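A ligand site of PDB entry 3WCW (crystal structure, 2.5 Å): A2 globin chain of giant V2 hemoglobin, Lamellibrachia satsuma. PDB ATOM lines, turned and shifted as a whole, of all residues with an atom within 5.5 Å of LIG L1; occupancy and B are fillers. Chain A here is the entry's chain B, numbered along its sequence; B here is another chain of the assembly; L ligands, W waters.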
ATOM      1  N   TRP A  33       4.508 -33.949  29.725  1.00  0.00           N
ATOM      2  CA  TRP A  33       5.595 -34.709  30.320  1.00  0.00           C
ATOM      3  C   TRP A  33       5.218 -35.884  31.203  1.00  0.00           C
ATOM      4  O   TRP A  33       6.012 -36.819  31.364  1.00  0.00           O
ATOM      5  CB  TRP A  33       6.538 -33.769  31.063  1.00  0.00           C
ATOM      6  CG  TRP A  33       7.373 -33.027  30.099  1.00  0.00           C
ATOM      7  CD1 TRP A  33       7.191 -31.753  29.668  1.00  0.00           C
ATOM      8  CD2 TRP A  33       8.490 -33.547  29.386  1.00  0.00           C
ATOM      9  NE1 TRP A  33       8.131 -31.447  28.712  1.00  0.00           N
ATOM     10  CE2 TRP A  33       8.945 -32.526  28.524  1.00  0.00           C
ATOM     11  CE3 TRP A  33       9.148 -34.783  29.385  1.00  0.00           C
ATOM     12  CZ2 TRP A  33      10.032 -32.698  27.666  1.00  0.00           C
ATOM     13  CZ3 TRP A  33      10.246 -34.960  28.533  1.00  0.00           C
ATOM     14  CH2 TRP A  33      10.669 -33.916  27.683  1.00  0.00           C
ATOM     15  N   ALA A  43      13.656 -42.286  29.942  1.00  0.00           N
ATOM     16  CA  ALA A  43      14.007 -40.954  29.444  1.00  0.00           C
ATOM     17  C   ALA A  43      14.401 -39.973  30.541  1.00  0.00           C
ATOM     18  O   ALA A  43      15.126 -39.006  30.288  1.00  0.00           O
ATOM     19  CB  ALA A  43      12.840 -40.394  28.640  1.00  0.00           C
ATOM     20  N   MET A  46      18.020 -38.460  31.461  1.00  0.00           N
ATOM     21  CA  MET A  46      18.606 -37.366  30.689  1.00  0.00           C
ATOM     22  C   MET A  46      18.349 -35.986  31.279  1.00  0.00           C
ATOM     23  O   MET A  46      18.997 -35.011  30.905  1.00  0.00           O
ATOM     24  CB  MET A  46      18.093 -37.403  29.242  1.00  0.00           C
ATOM     25  CG  MET A  46      18.614 -38.581  28.436  1.00  0.00           C
ATOM     26  SD  MET A  46      17.830 -38.712  26.826  1.00  0.00           S
ATOM     27  CE  MET A  46      18.619 -37.338  25.959  1.00  0.00           C
ATOM     28  N   PHE A  47      17.405 -35.915  32.218  1.00  0.00           N
ATOM     29  CA  PHE A  47      17.055 -34.647  32.829  1.00  0.00           C
ATOM     30  C   PHE A  47      17.470 -34.536  34.291  1.00  0.00           C
ATOM     31  O   PHE A  47      16.817 -33.852  35.067  1.00  0.00           O
ATOM     32  CB  PHE A  47      15.533 -34.444  32.734  1.00  0.00           C
ATOM     33  CG  PHE A  47      14.992 -34.559  31.338  1.00  0.00           C
ATOM     34  CD1 PHE A  47      14.938 -33.444  30.505  1.00  0.00           C
ATOM     35  CD2 PHE A  47      14.491 -35.773  30.870  1.00  0.00           C
ATOM     36  CE1 PHE A  47      14.400 -33.537  29.239  1.00  0.00           C
ATOM     37  CE2 PHE A  47      13.949 -35.868  29.595  1.00  0.00           C
ATOM     38  CZ  PHE A  47      13.904 -34.750  28.780  1.00  0.00           C
ATOM     39  N   ARG A  49      19.639 -32.814  35.624  1.00  0.00           N
ATOM     40  CA  ARG A  49      19.962 -31.444  36.043  1.00  0.00           C
ATOM     41  C   ARG A  49      18.737 -30.608  36.382  1.00  0.00           C
ATOM     42  O   ARG A  49      18.819 -29.664  37.179  1.00  0.00           O
ATOM     43  CB  ARG A  49      20.745 -30.725  34.950  1.00  0.00           C
ATOM     44  CG  ARG A  49      21.313 -29.388  35.420  1.00  0.00           C
ATOM     45  CD  ARG A  49      21.950 -28.620  34.280  1.00  0.00           C
ATOM     46  NE  ARG A  49      20.959 -27.984  33.406  1.00  0.00           N
ATOM     47  CZ  ARG A  49      20.208 -26.953  33.775  1.00  0.00           C
ATOM     48  NH1 ARG A  49      20.338 -26.442  34.986  1.00  0.00           N
ATOM     49  NH2 ARG A  49      19.340 -26.420  32.925  1.00  0.00           N
ATOM     50  N   VAL A  50      17.603 -30.945  35.782  1.00  0.00           N
ATOM     51  CA  VAL A  50      16.374 -30.200  36.001  1.00  0.00           C
ATOM     52  C   VAL A  50      15.304 -31.054  36.685  1.00  0.00           C
ATOM     53  O   VAL A  50      14.109 -30.971  36.375  1.00  0.00           O
ATOM     54  CB  VAL A  50      15.852 -29.627  34.648  1.00  0.00           C
ATOM     55  CG1 VAL A  50      16.903 -28.703  34.042  1.00  0.00           C
ATOM     56  CG2 VAL A  50      15.549 -30.752  33.677  1.00  0.00           C
ATOM     57  N   HIS A  63      11.965 -26.158  33.050  1.00  0.00           N
ATOM     58  CA  HIS A  63      12.426 -26.901  31.883  1.00  0.00           C
ATOM     59  C   HIS A  63      11.251 -27.028  30.916  1.00  0.00           C
ATOM     60  O   HIS A  63      11.359 -26.659  29.729  1.00  0.00           O
ATOM     61  CB  HIS A  63      12.927 -28.295  32.273  1.00  0.00           C
ATOM     62  CG  HIS A  63      13.149 -29.200  31.097  1.00  0.00           C
ATOM     63  ND1 HIS A  63      14.119 -28.950  30.147  1.00  0.00           N
ATOM     64  CD2 HIS A  63      12.448 -30.268  30.650  1.00  0.00           C
ATOM     65  CE1 HIS A  63      14.004 -29.832  29.163  1.00  0.00           C
ATOM     66  NE2 HIS A  63      12.996 -30.645  29.444  1.00  0.00           N
ATOM     67  N   ARG A  66      10.668 -24.057  29.026  1.00  0.00           N
ATOM     68  CA  ARG A  66      11.563 -23.786  27.906  1.00  0.00           C
ATOM     69  C   ARG A  66      11.213 -24.625  26.671  1.00  0.00           C
ATOM     70  O   ARG A  66      11.238 -24.131  25.551  1.00  0.00           O
ATOM     71  CB  ARG A  66      13.023 -24.016  28.310  1.00  0.00           C
ATOM     72  CG  ARG A  66      13.576 -22.957  29.222  1.00  0.00           C
ATOM     73  CD  ARG A  66      15.049 -23.181  29.493  1.00  0.00           C
ATOM     74  NE  ARG A  66      15.293 -24.360  30.319  1.00  0.00           N
ATOM     75  CZ  ARG A  66      15.282 -24.348  31.641  1.00  0.00           C
ATOM     76  NH1 ARG A  66      15.507 -25.475  32.309  1.00  0.00           N
ATOM     77  NH2 ARG A  66      15.053 -23.229  32.296  1.00  0.00           N
ATOM     78  N   VAL A  67      10.890 -25.897  26.884  1.00  0.00           N
ATOM     79  CA  VAL A  67      10.534 -26.792  25.787  1.00  0.00           C
ATOM     80  C   VAL A  67       9.322 -26.250  25.009  1.00  0.00           C
ATOM     81  O   VAL A  67       9.342 -26.198  23.773  1.00  0.00           O
ATOM     82  CB  VAL A  67      10.179 -28.223  26.293  1.00  0.00           C
ATOM     83  CG1 VAL A  67       9.729 -29.097  25.115  1.00  0.00           C
ATOM     84  CG2 VAL A  67      11.380 -28.835  26.997  1.00  0.00           C
ATOM     85  N   GLY A  70      10.086 -23.509  23.012  1.00  0.00           N
ATOM     86  CA  GLY A  70      10.791 -23.974  21.831  1.00  0.00           C
ATOM     87  C   GLY A  70       9.800 -24.281  20.721  1.00  0.00           C
ATOM     88  O   GLY A  70       9.972 -23.822  19.600  1.00  0.00           O
ATOM     89  N   LEU A  71       8.775 -25.067  21.040  1.00  0.00           N
ATOM     90  CA  LEU A  71       7.754 -25.409  20.065  1.00  0.00           C
ATOM     91  C   LEU A  71       7.050 -24.148  19.575  1.00  0.00           C
ATOM     92  O   LEU A  71       6.826 -23.982  18.388  1.00  0.00           O
ATOM     93  CB  LEU A  71       6.709 -26.354  20.672  1.00  0.00           C
ATOM     94  CG  LEU A  71       7.012 -27.845  20.793  1.00  0.00           C
ATOM     95  CD1 LEU A  71       5.927 -28.504  21.656  1.00  0.00           C
ATOM     96  CD2 LEU A  71       7.076 -28.478  19.402  1.00  0.00           C
ATOM     97  N   CYS A  74       9.041 -22.416  16.938  1.00  0.00           N
ATOM     98  CA  CYS A  74       9.009 -23.123  15.666  1.00  0.00           C
ATOM     99  C   CYS A  74       7.649 -23.002  14.990  1.00  0.00           C
ATOM    100  O   CYS A  74       7.572 -22.656  13.800  1.00  0.00           O
ATOM    101  CB  CYS A  74       9.333 -24.597  15.842  1.00  0.00           C
ATOM    102  SG  CYS A  74      10.992 -24.885  16.495  1.00  0.00           S
ATOM    103  N   LEU A  91      18.046 -25.122  18.212  1.00  0.00           N
ATOM    104  CA  LEU A  91      17.538 -26.196  19.054  1.00  0.00           C
ATOM    105  C   LEU A  91      18.370 -27.462  18.820  1.00  0.00           C
ATOM    106  O   LEU A  91      18.637 -28.208  19.754  1.00  0.00           O
ATOM    107  CB  LEU A  91      16.068 -26.467  18.741  1.00  0.00           C
ATOM    108  CG  LEU A  91      15.068 -25.349  19.041  1.00  0.00           C
ATOM    109  CD1 LEU A  91      13.697 -25.719  18.512  1.00  0.00           C
ATOM    110  CD2 LEU A  91      15.006 -25.077  20.538  1.00  0.00           C
ATOM    111  N   GLN A  94      21.416 -27.243  20.994  1.00  0.00           N
ATOM    112  CA  GLN A  94      21.079 -27.435  22.393  1.00  0.00           C
ATOM    113  C   GLN A  94      20.886 -28.903  22.754  1.00  0.00           C
ATOM    114  O   GLN A  94      20.914 -29.259  23.926  1.00  0.00           O
ATOM    115  CB  GLN A  94      19.852 -26.575  22.740  1.00  0.00           C
ATOM    116  CG  GLN A  94      20.068 -25.086  22.421  1.00  0.00           C
ATOM    117  CD  GLN A  94      18.837 -24.193  22.628  1.00  0.00           C
ATOM    118  OE1 GLN A  94      17.781 -24.422  22.026  1.00  0.00           O
ATOM    119  NE2 GLN A  94      18.974 -23.189  23.477  1.00  0.00           N
ATOM    120  N   HIS A  95      20.703 -29.754  21.743  1.00  0.00           N
ATOM    121  CA  HIS A  95      20.509 -31.192  21.940  1.00  0.00           C
ATOM    122  C   HIS A  95      21.632 -32.072  21.388  1.00  0.00           C
ATOM    123  O   HIS A  95      21.904 -33.136  21.919  1.00  0.00           O
ATOM    124  CB  HIS A  95      19.212 -31.669  21.289  1.00  0.00           C
ATOM    125  CG  HIS A  95      17.971 -31.113  21.922  1.00  0.00           C
ATOM    126  ND1 HIS A  95      17.577 -29.800  21.775  1.00  0.00           N
ATOM    127  CD2 HIS A  95      17.019 -31.701  22.692  1.00  0.00           C
ATOM    128  CE1 HIS A  95      16.446 -29.608  22.414  1.00  0.00           C
ATOM    129  NE2 HIS A  95      16.089 -30.734  22.982  1.00  0.00           N
ATOM    130  N   ARG A  98      23.348 -34.651  23.517  1.00  0.00           N
ATOM    131  CA  ARG A  98      22.591 -35.434  24.483  1.00  0.00           C
ATOM    132  C   ARG A  98      22.131 -36.836  24.094  1.00  0.00           C
ATOM    133  O   ARG A  98      21.556 -37.543  24.907  1.00  0.00           O
ATOM    134  CB  ARG A  98      21.410 -34.582  24.955  1.00  0.00           C
ATOM    135  CG  ARG A  98      21.881 -33.222  25.482  1.00  0.00           C
ATOM    136  CD  ARG A  98      20.742 -32.294  25.851  1.00  0.00           C
ATOM    137  NE  ARG A  98      21.215 -30.999  26.331  1.00  0.00           N
ATOM    138  CZ  ARG A  98      21.847 -30.795  27.484  1.00  0.00           C
ATOM    139  NH1 ARG A  98      22.238 -29.574  27.825  1.00  0.00           N
ATOM    140  NH2 ARG A  98      22.080 -31.809  28.310  1.00  0.00           N
ATOM    141  N   VAL A 100      19.722 -38.066  21.811  1.00  0.00           N
ATOM    142  CA  VAL A 100      18.272 -38.252  21.746  1.00  0.00           C
ATOM    143  C   VAL A 100      17.904 -39.194  20.583  1.00  0.00           C
ATOM    144  O   VAL A 100      18.156 -38.884  19.424  1.00  0.00           O
ATOM    145  CB  VAL A 100      17.568 -36.883  21.555  1.00  0.00           C
ATOM    146  CG1 VAL A 100      16.071 -37.049  21.613  1.00  0.00           C
ATOM    147  CG2 VAL A 100      18.049 -35.900  22.619  1.00  0.00           C
ATOM    148  N   GLN A 104      12.552 -41.479  20.992  1.00  0.00           N
ATOM    149  CA  GLN A 104      12.181 -40.529  22.021  1.00  0.00           C
ATOM    150  C   GLN A 104      11.530 -39.301  21.372  1.00  0.00           C
ATOM    151  O   GLN A 104      10.500 -38.820  21.853  1.00  0.00           O
ATOM    152  CB  GLN A 104      13.423 -40.127  22.827  1.00  0.00           C
ATOM    153  CG  GLN A 104      14.144 -41.306  23.465  1.00  0.00           C
ATOM    154  CD  GLN A 104      15.359 -40.894  24.294  1.00  0.00           C
ATOM    155  OE1 GLN A 104      16.286 -40.239  23.798  1.00  0.00           O
ATOM    156  NE2 GLN A 104      15.367 -41.283  25.573  1.00  0.00           N
ATOM    157  N   TYR A 105      12.116 -38.805  20.282  1.00  0.00           N
ATOM    158  CA  TYR A 105      11.548 -37.646  19.603  1.00  0.00           C
ATOM    159  C   TYR A 105      10.107 -37.984  19.229  1.00  0.00           C
ATOM    160  O   TYR A 105       9.227 -37.123  19.318  1.00  0.00           O
ATOM    161  CB  TYR A 105      12.351 -37.279  18.332  1.00  0.00           C
ATOM    162  CG  TYR A 105      13.556 -36.380  18.560  1.00  0.00           C
ATOM    163  CD1 TYR A 105      13.407 -35.063  19.026  1.00  0.00           C
ATOM    164  CD2 TYR A 105      14.860 -36.840  18.322  1.00  0.00           C
ATOM    165  CE1 TYR A 105      14.514 -34.248  19.263  1.00  0.00           C
ATOM    166  CE2 TYR A 105      15.970 -36.035  18.547  1.00  0.00           C
ATOM    167  CZ  TYR A 105      15.797 -34.739  19.018  1.00  0.00           C
ATOM    168  OH  TYR A 105      16.915 -33.958  19.265  1.00  0.00           O
ATOM    169  N   VAL A 108       7.914 -37.815  22.440  1.00  0.00           N
ATOM    170  CA  VAL A 108       7.619 -36.450  22.814  1.00  0.00           C
ATOM    171  C   VAL A 108       6.644 -35.844  21.801  1.00  0.00           C
ATOM    172  O   VAL A 108       5.849 -34.962  22.138  1.00  0.00           O
ATOM    173  CB  VAL A 108       8.921 -35.649  22.918  1.00  0.00           C
ATOM    174  CG1 VAL A 108       8.620 -34.172  23.105  1.00  0.00           C
ATOM    175  CG2 VAL A 108       9.745 -36.181  24.076  1.00  0.00           C
ATOM    176  N   VAL A 112       3.062 -34.351  22.953  1.00  0.00           N
ATOM    177  CA  VAL A 112       2.623 -33.029  22.521  1.00  0.00           C
ATOM    178  C   VAL A 112       1.275 -33.073  21.799  1.00  0.00           C
ATOM    179  O   VAL A 112       0.416 -32.216  22.026  1.00  0.00           O
ATOM    180  CB  VAL A 112       3.680 -32.378  21.606  1.00  0.00           C
ATOM    181  CG1 VAL A 112       3.120 -31.104  20.971  1.00  0.00           C
ATOM    182  CG2 VAL A 112       4.948 -32.062  22.413  1.00  0.00           C
ATOM    183  N   ILE A 137       9.504 -30.435  12.339  1.00  0.00           N
ATOM    184  CA  ILE A 137      10.199 -29.760  13.436  1.00  0.00           C
ATOM    185  C   ILE A 137      11.240 -30.640  14.131  1.00  0.00           C
ATOM    186  O   ILE A 137      12.330 -30.171  14.447  1.00  0.00           O
ATOM    187  CB  ILE A 137       9.195 -29.219  14.484  1.00  0.00           C
ATOM    188  CG1 ILE A 137       8.274 -28.190  13.815  1.00  0.00           C
ATOM    189  CG2 ILE A 137       9.951 -28.581  15.659  1.00  0.00           C
ATOM    190  CD1 ILE A 137       7.299 -27.489  14.753  1.00  0.00           C
ATOM    191  N   THR A 138      10.894 -31.899  14.376  1.00  0.00           N
ATOM    192  CA  THR A 138      11.834 -32.811  15.016  1.00  0.00           C
ATOM    193  C   THR A 138      13.010 -33.046  14.077  1.00  0.00           C
ATOM    194  O   THR A 138      14.168 -32.989  14.496  1.00  0.00           O
ATOM    195  CB  THR A 138      11.187 -34.187  15.389  1.00  0.00           C
ATOM    196  OG1 THR A 138      10.319 -34.605  14.337  1.00  0.00           O
ATOM    197  CG2 THR A 138      10.372 -34.085  16.677  1.00  0.00           C
ATOM    198  N   ILE A 141      15.497 -30.505  14.413  1.00  0.00           N
ATOM    199  CA  ILE A 141      16.216 -30.633  15.680  1.00  0.00           C
ATOM    200  C   ILE A 141      17.318 -31.693  15.637  1.00  0.00           C
ATOM    201  O   ILE A 141      18.342 -31.551  16.315  1.00  0.00           O
ATOM    202  CB  ILE A 141      15.265 -31.032  16.851  1.00  0.00           C
ATOM    203  CG1 ILE A 141      14.020 -30.141  16.871  1.00  0.00           C
ATOM    204  CG2 ILE A 141      16.028 -30.936  18.171  1.00  0.00           C
ATOM    205  CD1 ILE A 141      14.190 -28.836  17.597  1.00  0.00           C
ATOM    206  N   HIS B  94      18.284 -19.946  34.989  1.00  0.00           N
ATOM    207  CA  HIS B  94      18.740 -20.524  33.739  1.00  0.00           C
ATOM    208  C   HIS B  94      19.090 -19.421  32.734  1.00  0.00           C
ATOM    209  O   HIS B  94      19.995 -19.586  31.923  1.00  0.00           O
ATOM    210  CB  HIS B  94      17.663 -21.419  33.149  1.00  0.00           C
ATOM    211  CG  HIS B  94      18.103 -22.165  31.924  1.00  0.00           C
ATOM    212  ND1 HIS B  94      18.905 -23.282  31.987  1.00  0.00           N
ATOM    213  CD2 HIS B  94      17.855 -21.943  30.604  1.00  0.00           C
ATOM    214  CE1 HIS B  94      19.120 -23.722  30.758  1.00  0.00           C
ATOM    215  NE2 HIS B  94      18.495 -22.929  29.909  1.00  0.00           N
ATOM    216  N   GLN B  98      22.942 -18.176  31.182  1.00  0.00           N
ATOM    217  CA  GLN B  98      23.036 -18.016  29.730  1.00  0.00           C
ATOM    218  C   GLN B  98      23.691 -16.670  29.392  1.00  0.00           C
ATOM    219  O   GLN B  98      24.318 -16.539  28.343  1.00  0.00           O
ATOM    220  CB  GLN B  98      21.669 -18.079  29.067  1.00  0.00           C
ATOM    221  CG  GLN B  98      21.036 -19.467  29.026  1.00  0.00           C
ATOM    222  CD  GLN B  98      19.812 -19.523  28.141  1.00  0.00           C
ATOM    223  OE1 GLN B  98      18.958 -18.644  28.201  1.00  0.00           O
ATOM    224  NE2 GLN B  98      19.716 -20.555  27.331  1.00  0.00           N
HETATM  225  C1  LIG L   1      16.626 -29.016  26.597  1.00  0.00           C
HETATM  226  C2  LIG L   1      13.449 -27.929  23.279  1.00  0.00           C
HETATM  227  C3  LIG L   1      12.677 -32.604  22.404  1.00  0.00           C
HETATM  228  C4  LIG L   1      15.892 -33.673  25.825  1.00  0.00           C
HETATM  229  C5  LIG L   1      15.824 -28.299  25.772  1.00  0.00           C
HETATM  230  C6  LIG L   1      15.787 -26.894  25.768  1.00  0.00           C
HETATM  231  C7  LIG L   1      14.885 -26.569  24.834  1.00  0.00           C
HETATM  232  C8  LIG L   1      14.355 -27.790  24.246  1.00  0.00           C
HETATM  233  C9  LIG L   1      14.445 -25.143  24.419  1.00  0.00           C
HETATM  234  C10 LIG L   1      16.588 -25.948  26.639  1.00  0.00           C
HETATM  235  C11 LIG L   1      17.962 -25.673  26.080  1.00  0.00           C
HETATM  236  C12 LIG L   1      18.787 -24.733  26.952  1.00  0.00           C
HETATM  237  O1  LIG L   1      18.437 -23.529  27.051  1.00  0.00           O
HETATM  238  O2  LIG L   1      19.733 -25.195  27.534  1.00  0.00           O
HETATM  239  C13 LIG L   1      12.942 -29.109  22.717  1.00  0.00           C
HETATM  240  C14 LIG L   1      11.946 -29.127  21.663  1.00  0.00           C
HETATM  241  C15 LIG L   1      11.730 -30.527  21.398  1.00  0.00           C
HETATM  242  C16 LIG L   1      12.577 -31.215  22.309  1.00  0.00           C
HETATM  243  C17 LIG L   1      11.315 -27.949  21.013  1.00  0.00           C
HETATM  244  C18 LIG L   1      10.803 -31.000  20.409  1.00  0.00           C
HETATM  245  C19 LIG L   1       9.648 -31.550  20.687  1.00  0.00           C
HETATM  246  C20 LIG L   1      13.489 -33.299  23.277  1.00  0.00           C
HETATM  247  C21 LIG L   1      13.515 -34.766  23.332  1.00  0.00           C
HETATM  248  C22 LIG L   1      14.444 -35.124  24.325  1.00  0.00           C
HETATM  249  C23 LIG L   1      14.953 -33.795  24.838  1.00  0.00           C
HETATM  250  C24 LIG L   1      12.679 -35.714  22.456  1.00  0.00           C
HETATM  251  C25 LIG L   1      14.787 -36.374  24.726  1.00  0.00           C
HETATM  252  C26 LIG L   1      14.233 -37.372  25.340  1.00  0.00           C
HETATM  253  C27 LIG L   1      16.388 -32.488  26.334  1.00  0.00           C
HETATM  254  C28 LIG L   1      17.434 -32.398  27.430  1.00  0.00           C
HETATM  255  C29 LIG L   1      17.622 -31.068  27.619  1.00  0.00           C
HETATM  256  C30 LIG L   1      16.726 -30.362  26.685  1.00  0.00           C
HETATM  257  C31 LIG L   1      18.090 -33.577  28.113  1.00  0.00           C
HETATM  258  C32 LIG L   1      18.564 -30.404  28.591  1.00  0.00           C
HETATM  259  C33 LIG L   1      17.901 -29.935  29.840  1.00  0.00           C
HETATM  260  C34 LIG L   1      18.853 -29.283  30.741  1.00  0.00           C
HETATM  261  O3  LIG L   1      19.007 -28.013  30.696  1.00  0.00           O
HETATM  262  O4  LIG L   1      19.507 -29.984  31.537  1.00  0.00           O
HETATM  263  N1  LIG L   1      14.955 -28.875  24.850  1.00  0.00           N
HETATM  264  N2  LIG L   1      13.332 -30.330  23.112  1.00  0.00           N
HETATM  265  N3  LIG L   1      14.365 -32.758  24.201  1.00  0.00           N
HETATM  266  N4  LIG L   1      16.011 -31.253  25.931  1.00  0.00           N
HETATM  267 FE1  LIG L   1      14.666 -30.817  24.523  1.00  0.00          FE
HETATM  268  O1  LG2 L   2      13.483 -30.924  25.865  1.00  0.00           O
HETATM  269  O2  LG2 L   2      13.198 -31.696  26.791  1.00  0.00           O
HETATM  270  C1  LG3 L   3      21.036 -14.525  24.534  1.00  0.00           C
HETATM  271  C2  LG3 L   3      16.933 -13.269  26.516  1.00  0.00           C
HETATM  272  C3  LG3 L   3      18.775  -8.972  27.703  1.00  0.00           C
HETATM  273  C4  LG3 L   3      22.925 -10.311  25.733  1.00  0.00           C
HETATM  274  C5  LG3 L   3      19.750 -14.584  24.965  1.00  0.00           C
HETATM  275  C6  LG3 L   3      18.915 -15.684  24.763  1.00  0.00           C
HETATM  276  C7  LG3 L   3      17.736 -15.353  25.334  1.00  0.00           C
HETATM  277  C8  LG3 L   3      17.851 -13.997  25.896  1.00  0.00           C
HETATM  278  C9  LG3 L   3      16.445 -16.204  25.403  1.00  0.00           C
HETATM  279  C10 LG3 L   3      19.264 -16.992  24.045  1.00  0.00           C
HETATM  280  C11 LG3 L   3      19.838 -18.042  24.941  1.00  0.00           C
HETATM  281  C12 LG3 L   3      20.200 -19.351  24.217  1.00  0.00           C
HETATM  282  O1  LG3 L   3      19.311 -19.998  23.601  1.00  0.00           O
HETATM  283  O2  LG3 L   3      21.349 -19.695  24.254  1.00  0.00           O
HETATM  284  C13 LG3 L   3      17.033 -11.956  27.037  1.00  0.00           C
HETATM  285  C14 LG3 L   3      15.947 -11.245  27.689  1.00  0.00           C
HETATM  286  C15 LG3 L   3      16.517  -9.965  28.031  1.00  0.00           C
HETATM  287  C16 LG3 L   3      17.863 -10.010  27.575  1.00  0.00           C
HETATM  288  C17 LG3 L   3      14.569 -11.760  27.927  1.00  0.00           C
HETATM  289  C18 LG3 L   3      15.781  -8.906  28.694  1.00  0.00           C
HETATM  290  C19 LG3 L   3      15.528  -8.878  29.991  1.00  0.00           C
HETATM  291  C20 LG3 L   3      20.080  -8.977  27.273  1.00  0.00           C
HETATM  292  C21 LG3 L   3      20.975  -7.821  27.458  1.00  0.00           C
HETATM  293  C22 LG3 L   3      22.219  -8.174  26.879  1.00  0.00           C
HETATM  294  C23 LG3 L   3      21.975  -9.587  26.370  1.00  0.00           C
HETATM  295  C24 LG3 L   3      20.590  -6.506  28.136  1.00  0.00           C
HETATM  296  C25 LG3 L   3      23.375  -7.420  26.794  1.00  0.00           C
HETATM  297  C26 LG3 L   3      23.849  -6.240  27.100  1.00  0.00           C
HETATM  298  C27 LG3 L   3      22.777 -11.587  25.220  1.00  0.00           C
HETATM  299  C28 LG3 L   3      23.869 -12.339  24.492  1.00  0.00           C
HETATM  300  C29 LG3 L   3      23.282 -13.530  24.166  1.00  0.00           C
HETATM  301  C30 LG3 L   3      21.912 -13.506  24.672  1.00  0.00           C
HETATM  302  C31 LG3 L   3      25.274 -11.807  24.225  1.00  0.00           C
HETATM  303  C32 LG3 L   3      23.885 -14.687  23.394  1.00  0.00           C
HETATM  304  C33 LG3 L   3      23.483 -14.551  21.952  1.00  0.00           C
HETATM  305  C34 LG3 L   3      23.950 -15.629  21.100  1.00  0.00           C
HETATM  306  O3  LG3 L   3      25.156 -15.650  20.712  1.00  0.00           O
HETATM  307  O4  LG3 L   3      23.149 -16.520  20.777  1.00  0.00           O
HETATM  308  N1  LG3 L   3      19.115 -13.540  25.659  1.00  0.00           N
HETATM  309  N2  LG3 L   3      18.161 -11.252  26.952  1.00  0.00           N
HETATM  310  N3  LG3 L   3      20.721 -10.013  26.620  1.00  0.00           N
HETATM  311  N4  LG3 L   3      21.650 -12.328  25.299  1.00  0.00           N
HETATM  312 FE1  LG3 L   3      19.922 -11.789  26.151  1.00  0.00          FE
HETATM  313  O   HOH W   1      19.516 -32.726  32.591  1.00  0.00           O
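NE2 of His 63 lies within hydrogen-bond range of O2 of LG2 L2 (2.9 Å).
NE2 of Gln 94 of chain A is in hydrogen-bond range of O1 of LG3 L3 (3.2 Å).
FE1 of LIG L1 is bound by NE2 of His 95.
The side-chain amide nitrogen (NE2) of Gln 98 of chain B lies within hydrogen-bond range of an oxygen (O1) of LIG L1, at 3.2 Å.
NH2 of Arg 49 is in salt-bridge range of O3 of LIG L1.
NE2 of His 94 of chain B is in hydrogen-bond range of O1 of LIG L1 (2.9 Å).
An oxygen (O1) of LG2 L2 is bound to an iron atom (FE1) of LIG L1 (1.8 Å).
ND1 of His 95 sits at hydrogen-bond distance from O of Leu 91.
The backbone carbonyl oxygen of Gln 94 of chain A sits at hydrogen-bond distance from the guanidinium group of Arg 98 of chain A (3.0 Å).
The guanidinium group (NH2) of Arg 49 lies within hydrogen-bond range of a ring nitrogen (ND1) of His 94 of chain B, 3.3 Å away.
OE1 of Gln 104 sits close to SD of Met 46 (3.7 Å).
The backbone carbonyl oxygen of Gly 70 sits at hydrogen-bond distance from the side-chain sulfur of Cys 74, at 3.4 Å.
Met 46 touches LIG L1 (O to C31, 3.3 Å).
Phe 47 touches LIG L1.
CG1 of Val 50 touches O4 of LIG L1 (3.8 Å).
His 63 touches LIG L1 (CE1 to C30, 3.7 Å).
Arg 66 touches LIG L1 (O to C9, 3.5 Å).
Val 67 touches LIG L1.
Gly 70 touches LIG L1 (C to C17, 3.98 Å).
Leu 71 touches LIG L1 (N to C17, 3.8 Å).
Leu 91 touches LIG L1.
Gln 94 of chain A touches LIG L1 (NE2 to O1, 3.6 Å).
CZ of Arg 98 of chain A touches C32 of LIG L1 (3.5 Å).
Val 100 touches LIG L1.
Gln 104 touches LIG L1.
Tyr 105 touches LIG L1.
CG2 of Val 108 touches C24 of LIG L1, 3.4 Å away.
Of the 26 residues printed, 19 come within 4 Å of LIG L1.
Along chain A the residues within 4 Å of LIG L1 span positions 46 to 108.
Water W1 lies within hydrogen-bond range of O of Met 46 (2.9 Å), O4 of LIG L1 (2.9 Å) and N of Arg 49 (3.0 Å).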
